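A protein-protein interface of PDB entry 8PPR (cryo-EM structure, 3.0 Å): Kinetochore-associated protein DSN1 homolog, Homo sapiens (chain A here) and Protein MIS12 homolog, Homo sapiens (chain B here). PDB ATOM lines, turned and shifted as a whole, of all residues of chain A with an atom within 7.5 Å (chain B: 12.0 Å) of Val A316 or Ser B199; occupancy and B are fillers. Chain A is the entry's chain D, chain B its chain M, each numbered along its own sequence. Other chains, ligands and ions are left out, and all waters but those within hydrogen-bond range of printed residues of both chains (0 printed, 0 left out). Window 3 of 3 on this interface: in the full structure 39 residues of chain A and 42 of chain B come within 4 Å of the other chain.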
ATOM      1  N   THR A 310     -13.493 -22.011  21.228  1.00  0.00           N
ATOM      2  CA  THR A 310     -14.097 -20.921  20.473  1.00  0.00           C
ATOM      3  C   THR A 310     -13.505 -20.834  19.076  1.00  0.00           C
ATOM      4  O   THR A 310     -14.231 -20.618  18.097  1.00  0.00           O
ATOM      5  CB  THR A 310     -13.903 -19.599  21.214  1.00  0.00           C
ATOM      6  OG1 THR A 310     -14.512 -19.681  22.508  1.00  0.00           O
ATOM      7  CG2 THR A 310     -14.535 -18.456  20.435  1.00  0.00           C
ATOM      8  N   GLN A 311     -12.185 -20.993  18.963  1.00  0.00           N
ATOM      9  CA  GLN A 311     -11.559 -20.958  17.646  1.00  0.00           C
ATOM     10  C   GLN A 311     -12.085 -22.082  16.761  1.00  0.00           C
ATOM     11  O   GLN A 311     -12.367 -21.870  15.574  1.00  0.00           O
ATOM     12  CB  GLN A 311     -10.043 -21.049  17.788  1.00  0.00           C
ATOM     13  CG  GLN A 311      -9.414 -19.797  18.368  1.00  0.00           C
ATOM     14  CD  GLN A 311      -7.904 -19.883  18.423  1.00  0.00           C
ATOM     15  OE1 GLN A 311      -7.286 -20.619  17.656  1.00  0.00           O
ATOM     16  NE2 GLN A 311      -7.302 -19.127  19.333  1.00  0.00           N
ATOM     17  N   CYS A 312     -12.232 -23.281  17.326  1.00  0.00           N
ATOM     18  CA  CYS A 312     -12.775 -24.402  16.566  1.00  0.00           C
ATOM     19  C   CYS A 312     -14.200 -24.117  16.111  1.00  0.00           C
ATOM     20  O   CYS A 312     -14.563 -24.380  14.956  1.00  0.00           O
ATOM     21  CB  CYS A 312     -12.726 -25.675  17.411  1.00  0.00           C
ATOM     22  SG  CYS A 312     -13.662 -27.058  16.725  1.00  0.00           S
ATOM     23  N   PHE A 313     -15.025 -23.580  17.013  1.00  0.00           N
ATOM     24  CA  PHE A 313     -16.402 -23.258  16.652  1.00  0.00           C
ATOM     25  C   PHE A 313     -16.449 -22.245  15.520  1.00  0.00           C
ATOM     26  O   PHE A 313     -17.216 -22.405  14.566  1.00  0.00           O
ATOM     27  CB  PHE A 313     -17.159 -22.721  17.865  1.00  0.00           C
ATOM     28  CG  PHE A 313     -17.468 -23.761  18.896  1.00  0.00           C
ATOM     29  CD1 PHE A 313     -17.504 -25.102  18.556  1.00  0.00           C
ATOM     30  CD2 PHE A 313     -17.744 -23.397  20.202  1.00  0.00           C
ATOM     31  CE1 PHE A 313     -17.796 -26.062  19.504  1.00  0.00           C
ATOM     32  CE2 PHE A 313     -18.037 -24.352  21.154  1.00  0.00           C
ATOM     33  CZ  PHE A 313     -18.064 -25.687  20.805  1.00  0.00           C
ATOM     34  N   GLN A 314     -15.628 -21.199  15.608  1.00  0.00           N
ATOM     35  CA  GLN A 314     -15.620 -20.178  14.567  1.00  0.00           C
ATOM     36  C   GLN A 314     -15.165 -20.754  13.235  1.00  0.00           C
ATOM     37  O   GLN A 314     -15.732 -20.432  12.183  1.00  0.00           O
ATOM     38  CB  GLN A 314     -14.723 -19.017  14.983  1.00  0.00           C
ATOM     39  CG  GLN A 314     -15.240 -18.244  16.177  1.00  0.00           C
ATOM     40  CD  GLN A 314     -14.482 -16.956  16.402  1.00  0.00           C
ATOM     41  OE1 GLN A 314     -13.443 -16.719  15.785  1.00  0.00           O
ATOM     42  NE2 GLN A 314     -14.994 -16.113  17.290  1.00  0.00           N
ATOM     43  N   LYS A 315     -14.137 -21.605  13.257  1.00  0.00           N
ATOM     44  CA  LYS A 315     -13.648 -22.196  12.017  1.00  0.00           C
ATOM     45  C   LYS A 315     -14.715 -23.066  11.366  1.00  0.00           C
ATOM     46  O   LYS A 315     -14.946 -22.988  10.154  1.00  0.00           O
ATOM     47  CB  LYS A 315     -12.385 -23.009  12.289  1.00  0.00           C
ATOM     48  CG  LYS A 315     -11.923 -23.825  11.100  1.00  0.00           C
ATOM     49  CD  LYS A 315     -10.928 -24.883  11.526  1.00  0.00           C
ATOM     50  CE  LYS A 315     -11.587 -25.901  12.439  1.00  0.00           C
ATOM     51  NZ  LYS A 315     -12.554 -26.756  11.698  1.00  0.00           N
ATOM     52  N   VAL A 316     -15.386 -23.902  12.162  1.00  0.00           N
ATOM     53  CA  VAL A 316     -16.418 -24.752  11.579  1.00  0.00           C
ATOM     54  C   VAL A 316     -17.588 -23.909  11.090  1.00  0.00           C
ATOM     55  O   VAL A 316     -18.200 -24.220  10.060  1.00  0.00           O
ATOM     56  CB  VAL A 316     -16.869 -25.827  12.584  1.00  0.00           C
ATOM     57  CG1 VAL A 316     -17.910 -26.735  11.952  1.00  0.00           C
ATOM     58  CG2 VAL A 316     -15.678 -26.640  13.051  1.00  0.00           C
ATOM     59  N   SER A 317     -17.910 -22.826  11.800  1.00  0.00           N
ATOM     60  CA  SER A 317     -19.001 -21.958  11.371  1.00  0.00           C
ATOM     61  C   SER A 317     -18.693 -21.298  10.034  1.00  0.00           C
ATOM     62  O   SER A 317     -19.555 -21.248   9.151  1.00  0.00           O
ATOM     63  CB  SER A 317     -19.276 -20.903  12.439  1.00  0.00           C
ATOM     64  OG  SER A 317     -20.321 -20.035  12.040  1.00  0.00           O
ATOM     65  N   VAL A 318     -17.472 -20.789   9.864  1.00  0.00           N
ATOM     66  CA  VAL A 318     -17.136 -20.158   8.592  1.00  0.00           C
ATOM     67  C   VAL A 318     -17.049 -21.197   7.482  1.00  0.00           C
ATOM     68  O   VAL A 318     -17.396 -20.909   6.329  1.00  0.00           O
ATOM     69  CB  VAL A 318     -15.845 -19.322   8.708  1.00  0.00           C
ATOM     70  CG1 VAL A 318     -15.981 -18.298   9.822  1.00  0.00           C
ATOM     71  CG2 VAL A 318     -14.632 -20.203   8.936  1.00  0.00           C
ATOM     72  N   GLN A 319     -16.605 -22.420   7.795  1.00  0.00           N
ATOM     73  CA  GLN A 319     -16.624 -23.474   6.787  1.00  0.00           C
ATOM     74  C   GLN A 319     -18.046 -23.779   6.334  1.00  0.00           C
ATOM     75  O   GLN A 319     -18.309 -23.919   5.133  1.00  0.00           O
ATOM     76  CB  GLN A 319     -15.970 -24.741   7.326  1.00  0.00           C
ATOM     77  CG  GLN A 319     -16.058 -25.897   6.352  1.00  0.00           C
ATOM     78  CD  GLN A 319     -15.487 -27.179   6.906  1.00  0.00           C
ATOM     79  OE1 GLN A 319     -15.498 -28.210   6.237  1.00  0.00           O
ATOM     80  NE2 GLN A 319     -14.986 -27.126   8.134  1.00  0.00           N
ATOM     81  N   LEU A 320     -18.974 -23.894   7.284  1.00  0.00           N
ATOM     82  CA  LEU A 320     -20.367 -24.144   6.935  1.00  0.00           C
ATOM     83  C   LEU A 320     -20.942 -22.990   6.127  1.00  0.00           C
ATOM     84  O   LEU A 320     -21.694 -23.204   5.167  1.00  0.00           O
ATOM     85  CB  LEU A 320     -21.186 -24.374   8.201  1.00  0.00           C
ATOM     86  CG  LEU A 320     -22.646 -24.758   7.983  1.00  0.00           C
ATOM     87  CD1 LEU A 320     -22.731 -26.089   7.257  1.00  0.00           C
ATOM     88  CD2 LEU A 320     -23.376 -24.819   9.313  1.00  0.00           C
ATOM     89  N   GLY A 321     -20.599 -21.759   6.506  1.00  0.00           N
ATOM     90  CA  GLY A 321     -21.044 -20.611   5.739  1.00  0.00           C
ATOM     91  C   GLY A 321     -20.550 -20.650   4.307  1.00  0.00           C
ATOM     92  O   GLY A 321     -21.315 -20.405   3.377  1.00  0.00           O
ATOM     93  N   LYS A 322     -19.270 -20.974   4.113  1.00  0.00           N
ATOM     94  CA  LYS A 322     -18.725 -21.072   2.761  1.00  0.00           C
ATOM     95  C   LYS A 322     -19.398 -22.187   1.972  1.00  0.00           C
ATOM     96  O   LYS A 322     -19.668 -22.040   0.771  1.00  0.00           O
ATOM     97  CB  LYS A 322     -17.217 -21.302   2.823  1.00  0.00           C
ATOM     98  CG  LYS A 322     -16.532 -21.269   1.471  1.00  0.00           C
ATOM     99  CD  LYS A 322     -15.043 -21.523   1.613  1.00  0.00           C
ATOM    100  CE  LYS A 322     -14.353 -20.359   2.303  1.00  0.00           C
ATOM    101  NZ  LYS A 322     -14.385 -19.120   1.479  1.00  0.00           N
ATOM    102  N   LEU B 188     -18.450 -29.580  27.694  1.00  0.00           N
ATOM    103  CA  LEU B 188     -17.912 -28.899  26.526  1.00  0.00           C
ATOM    104  C   LEU B 188     -17.032 -29.822  25.699  1.00  0.00           C
ATOM    105  O   LEU B 188     -16.996 -29.700  24.474  1.00  0.00           O
ATOM    106  CB  LEU B 188     -17.128 -27.661  26.956  1.00  0.00           C
ATOM    107  CG  LEU B 188     -16.589 -26.796  25.817  1.00  0.00           C
ATOM    108  CD1 LEU B 188     -17.696 -26.467  24.831  1.00  0.00           C
ATOM    109  CD2 LEU B 188     -15.961 -25.526  26.360  1.00  0.00           C
ATOM    110  N   ASN B 190     -17.561 -33.054  25.366  1.00  0.00           N
ATOM    111  CA  ASN B 190     -18.525 -33.850  24.611  1.00  0.00           C
ATOM    112  C   ASN B 190     -19.069 -33.064  23.426  1.00  0.00           C
ATOM    113  O   ASN B 190     -19.182 -33.591  22.308  1.00  0.00           O
ATOM    114  CB  ASN B 190     -19.665 -34.286  25.527  1.00  0.00           C
ATOM    115  CG  ASN B 190     -19.232 -35.329  26.531  1.00  0.00           C
ATOM    116  OD1 ASN B 190     -18.373 -36.162  26.246  1.00  0.00           O
ATOM    117  ND2 ASN B 190     -19.818 -35.283  27.721  1.00  0.00           N
ATOM    118  N   ILE B 191     -19.404 -31.794  23.656  1.00  0.00           N
ATOM    119  CA  ILE B 191     -19.918 -30.946  22.585  1.00  0.00           C
ATOM    120  C   ILE B 191     -18.879 -30.797  21.483  1.00  0.00           C
ATOM    121  O   ILE B 191     -19.197 -30.876  20.292  1.00  0.00           O
ATOM    122  CB  ILE B 191     -20.341 -29.581  23.154  1.00  0.00           C
ATOM    123  CG1 ILE B 191     -21.572 -29.738  24.046  1.00  0.00           C
ATOM    124  CG2 ILE B 191     -20.617 -28.597  22.029  1.00  0.00           C
ATOM    125  CD1 ILE B 191     -21.962 -28.470  24.766  1.00  0.00           C
ATOM    126  N   ARG B 192     -17.621 -30.576  21.867  1.00  0.00           N
ATOM    127  CA  ARG B 192     -16.548 -30.420  20.893  1.00  0.00           C
ATOM    128  C   ARG B 192     -16.337 -31.700  20.102  1.00  0.00           C
ATOM    129  O   ARG B 192     -16.062 -31.652  18.901  1.00  0.00           O
ATOM    130  CB  ARG B 192     -15.257 -30.016  21.599  1.00  0.00           C
ATOM    131  CG  ARG B 192     -15.211 -28.565  22.020  1.00  0.00           C
ATOM    132  CD  ARG B 192     -13.781 -28.084  22.160  1.00  0.00           C
ATOM    133  NE  ARG B 192     -12.965 -28.448  21.009  1.00  0.00           N
ATOM    134  CZ  ARG B 192     -11.682 -28.138  20.874  1.00  0.00           C
ATOM    135  NH1 ARG B 192     -11.037 -27.451  21.803  1.00  0.00           N
ATOM    136  NH2 ARG B 192     -11.033 -28.524  19.780  1.00  0.00           N
ATOM    137  N   ASP B 193     -16.440 -32.852  20.764  1.00  0.00           N
ATOM    138  CA  ASP B 193     -16.306 -34.120  20.059  1.00  0.00           C
ATOM    139  C   ASP B 193     -17.408 -34.283  19.025  1.00  0.00           C
ATOM    140  O   ASP B 193     -17.146 -34.668  17.878  1.00  0.00           O
ATOM    141  CB  ASP B 193     -16.338 -35.271  21.061  1.00  0.00           C
ATOM    142  CG  ASP B 193     -15.130 -35.279  21.972  1.00  0.00           C
ATOM    143  OD1 ASP B 193     -14.195 -34.488  21.724  1.00  0.00           O
ATOM    144  OD2 ASP B 193     -15.119 -36.069  22.938  1.00  0.00           O
ATOM    145  N   ASN B 194     -18.648 -33.976  19.410  1.00  0.00           N
ATOM    146  CA  ASN B 194     -19.758 -34.059  18.465  1.00  0.00           C
ATOM    147  C   ASN B 194     -19.533 -33.109  17.294  1.00  0.00           C
ATOM    148  O   ASN B 194     -19.728 -33.476  16.127  1.00  0.00           O
ATOM    149  CB  ASN B 194     -21.068 -33.742  19.191  1.00  0.00           C
ATOM    150  CG  ASN B 194     -22.269 -33.670  18.259  1.00  0.00           C
ATOM    151  OD1 ASN B 194     -22.195 -34.017  17.080  1.00  0.00           O
ATOM    152  ND2 ASN B 194     -23.391 -33.205  18.794  1.00  0.00           N
ATOM    153  N   VAL B 195     -19.108 -31.881  17.595  1.00  0.00           N
ATOM    154  CA  VAL B 195     -18.897 -30.878  16.558  1.00  0.00           C
ATOM    155  C   VAL B 195     -17.798 -31.321  15.605  1.00  0.00           C
ATOM    156  O   VAL B 195     -17.924 -31.185  14.384  1.00  0.00           O
ATOM    157  CB  VAL B 195     -18.573 -29.516  17.200  1.00  0.00           C
ATOM    158  CG1 VAL B 195     -17.929 -28.583  16.187  1.00  0.00           C
ATOM    159  CG2 VAL B 195     -19.832 -28.896  17.783  1.00  0.00           C
ATOM    160  N   GLU B 196     -16.702 -31.851  16.146  1.00  0.00           N
ATOM    161  CA  GLU B 196     -15.602 -32.307  15.309  1.00  0.00           C
ATOM    162  C   GLU B 196     -16.030 -33.469  14.427  1.00  0.00           C
ATOM    163  O   GLU B 196     -15.668 -33.523  13.247  1.00  0.00           O
ATOM    164  CB  GLU B 196     -14.413 -32.705  16.179  1.00  0.00           C
ATOM    165  CG  GLU B 196     -13.532 -31.539  16.575  1.00  0.00           C
ATOM    166  CD  GLU B 196     -12.797 -30.949  15.391  1.00  0.00           C
ATOM    167  OE1 GLU B 196     -12.498 -31.702  14.440  1.00  0.00           O
ATOM    168  OE2 GLU B 196     -12.520 -29.732  15.409  1.00  0.00           O
ATOM    169  N   LYS B 197     -16.803 -34.405  14.979  1.00  0.00           N
ATOM    170  CA  LYS B 197     -17.281 -35.527  14.181  1.00  0.00           C
ATOM    171  C   LYS B 197     -18.158 -35.044  13.034  1.00  0.00           C
ATOM    172  O   LYS B 197     -17.995 -35.471  11.884  1.00  0.00           O
ATOM    173  CB  LYS B 197     -18.046 -36.505  15.068  1.00  0.00           C
ATOM    174  CG  LYS B 197     -18.346 -37.836  14.410  1.00  0.00           C
ATOM    175  CD  LYS B 197     -19.327 -38.641  15.243  1.00  0.00           C
ATOM    176  CE  LYS B 197     -18.828 -38.801  16.670  1.00  0.00           C
ATOM    177  NZ  LYS B 197     -17.478 -39.424  16.719  1.00  0.00           N
ATOM    178  N   GLU B 198     -19.088 -34.135  13.330  1.00  0.00           N
ATOM    179  CA  GLU B 198     -19.978 -33.635  12.288  1.00  0.00           C
ATOM    180  C   GLU B 198     -19.211 -32.835  11.242  1.00  0.00           C
ATOM    181  O   GLU B 198     -19.489 -32.946  10.041  1.00  0.00           O
ATOM    182  CB  GLU B 198     -21.088 -32.793  12.914  1.00  0.00           C
ATOM    183  CG  GLU B 198     -22.268 -33.617  13.396  1.00  0.00           C
ATOM    184  CD  GLU B 198     -23.186 -32.843  14.317  1.00  0.00           C
ATOM    185  OE1 GLU B 198     -22.885 -31.668  14.610  1.00  0.00           O
ATOM    186  OE2 GLU B 198     -24.210 -33.411  14.750  1.00  0.00           O
ATOM    187  N   SER B 199     -18.242 -32.028  11.676  1.00  0.00           N
ATOM    188  CA  SER B 199     -17.441 -31.254  10.737  1.00  0.00           C
ATOM    189  C   SER B 199     -16.616 -32.164   9.841  1.00  0.00           C
ATOM    190  O   SER B 199     -16.484 -31.909   8.640  1.00  0.00           O
ATOM    191  CB  SER B 199     -16.535 -30.286  11.493  1.00  0.00           C
ATOM    192  OG  SER B 199     -15.652 -29.622  10.606  1.00  0.00           O
ATOM    193  N   LYS B 200     -16.041 -33.223  10.409  1.00  0.00           N
ATOM    194  CA  LYS B 200     -15.293 -34.179   9.603  1.00  0.00           C
ATOM    195  C   LYS B 200     -16.199 -34.870   8.595  1.00  0.00           C
ATOM    196  O   LYS B 200     -15.812 -35.075   7.438  1.00  0.00           O
ATOM    197  CB  LYS B 200     -14.617 -35.204  10.511  1.00  0.00           C
ATOM    198  CG  LYS B 200     -13.948 -36.347   9.770  1.00  0.00           C
ATOM    199  CD  LYS B 200     -13.821 -37.573  10.658  1.00  0.00           C
ATOM    200  CE  LYS B 200     -13.119 -37.246  11.967  1.00  0.00           C
ATOM    201  NZ  LYS B 200     -11.890 -36.428  11.766  1.00  0.00           N
ATOM    202  N   ARG B 201     -17.410 -35.237   9.018  1.00  0.00           N
ATOM    203  CA  ARG B 201     -18.352 -35.862   8.096  1.00  0.00           C
ATOM    204  C   ARG B 201     -18.721 -34.914   6.962  1.00  0.00           C
ATOM    205  O   ARG B 201     -18.828 -35.331   5.803  1.00  0.00           O
ATOM    206  CB  ARG B 201     -19.601 -36.311   8.849  1.00  0.00           C
ATOM    207  CG  ARG B 201     -20.692 -36.862   7.955  1.00  0.00           C
ATOM    208  CD  ARG B 201     -21.908 -37.245   8.771  1.00  0.00           C
ATOM    209  NE  ARG B 201     -22.851 -36.139   8.872  1.00  0.00           N
ATOM    210  CZ  ARG B 201     -23.235 -35.589  10.015  1.00  0.00           C
ATOM    211  NH1 ARG B 201     -22.773 -36.019  11.178  1.00  0.00           N
ATOM    212  NH2 ARG B 201     -24.102 -34.581   9.991  1.00  0.00           N
ATOM    213  N   LEU B 202     -18.926 -33.636   7.278  1.00  0.00           N
ATOM    214  CA  LEU B 202     -19.212 -32.657   6.234  1.00  0.00           C
ATOM    215  C   LEU B 202     -18.017 -32.477   5.306  1.00  0.00           C
ATOM    216  O   LEU B 202     -18.186 -32.311   4.092  1.00  0.00           O
ATOM    217  CB  LEU B 202     -19.614 -31.323   6.860  1.00  0.00           C
ATOM    218  CG  LEU B 202     -20.931 -31.304   7.640  1.00  0.00           C
ATOM    219  CD1 LEU B 202     -21.504 -29.898   7.680  1.00  0.00           C
ATOM    220  CD2 LEU B 202     -21.938 -32.279   7.045  1.00  0.00           C
ATOM    221  N   LYS B 203     -16.805 -32.495   5.863  1.00  0.00           N
ATOM    222  CA  LYS B 203     -15.604 -32.354   5.048  1.00  0.00           C
ATOM    223  C   LYS B 203     -15.466 -33.505   4.065  1.00  0.00           C
ATOM    224  O   LYS B 203     -15.259 -33.287   2.865  1.00  0.00           O
ATOM    225  CB  LYS B 203     -14.372 -32.282   5.948  1.00  0.00           C
ATOM    226  CG  LYS B 203     -13.981 -30.882   6.362  1.00  0.00           C
ATOM    227  CD  LYS B 203     -12.634 -30.873   7.057  1.00  0.00           C
ATOM    228  CE  LYS B 203     -12.693 -31.631   8.371  1.00  0.00           C
ATOM    229  NZ  LYS B 203     -13.789 -31.132   9.244  1.00  0.00           N
ATOM    230  N   ILE B 204     -15.578 -34.741   4.554  1.00  0.00           N
ATOM    231  CA  ILE B 204     -15.449 -35.897   3.674  1.00  0.00           C
ATOM    232  C   ILE B 204     -16.626 -35.966   2.708  1.00  0.00           C
ATOM    233  O   ILE B 204     -16.472 -36.369   1.550  1.00  0.00           O
ATOM    234  CB  ILE B 204     -15.302 -37.190   4.499  1.00  0.00           C
ATOM    235  CG1 ILE B 204     -16.534 -37.427   5.372  1.00  0.00           C
ATOM    236  CG2 ILE B 204     -14.052 -37.126   5.363  1.00  0.00           C
ATOM    237  CD1 ILE B 204     -16.566 -38.786   6.032  1.00  0.00           C
ATOM    238  N   SER B 205     -17.811 -35.577   3.165  1.00  0.00           N
ATOM    239  CA  SER B 205     -19.005 -35.617   2.331  1.00  0.00           C
ATOM    240  C   SER B 205     -19.623 -34.230   2.193  1.00  0.00           C
ATOM    241  O   SER B 205     -20.802 -34.036   2.488  1.00  0.00           O
ATOM    242  CB  SER B 205     -20.025 -36.596   2.911  1.00  0.00           C
ATOM    243  OG  SER B 205     -20.111 -36.464   4.319  1.00  0.00           O
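The side-chain hydroxyl (OG) of Ser B199 lies within hydrogen-bond range of the side-chain amino group (NZ) of Lys B203, 2.8 Å away.
SG of Cys A312 lies within hydrogen-bond range of OE2 of Glu B196 (3.2 Å).
Phe A313 touches Val B195.
Ser B199 touches Val A316.
NE2 of Gln A319 touches OG of Ser B199, at 3.6 Å.
Lys B203 touches Gln A319.
Of the 17 printed residues of chain B, 4 touch a printed residue of chain A.
Hydrophobic or aromatic side chains of chain B that line the printed part of chain A: Val B195.
Hydrophobic or aromatic side chains of chain A within 4 Å of the printed part of chain B: Phe A313 and Val A316.
Along chain A the printed residues that touch a printed residue of chain B span positions 312 to 319.
Among the printed residues, 5 pairs touch across the chains.
Among the printed residues, no Asp or Glu carboxylate lies within 4 Å of a Lys or Arg side-chain nitrogen of the other chain.
Cys A312 touches just one residue of chain B: Glu B196 (3.2 Å).
No residue of chain B comes within 4 Å of Ser A317.
No residue of chain B comes within 4 Å of Val A318.
Of chain B, only Ser B199 and Lys B203 come within 4 Å of Gln A319.
Of the printed residues of chain A, Val B195 touches Phe A313 (3.9 Å).
Printed residues of chain A within 4 Å of Glu B196: Cys A312.
The nearest residue of chain B that does not touch Val A316 is Val B195 (4.3 Å).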
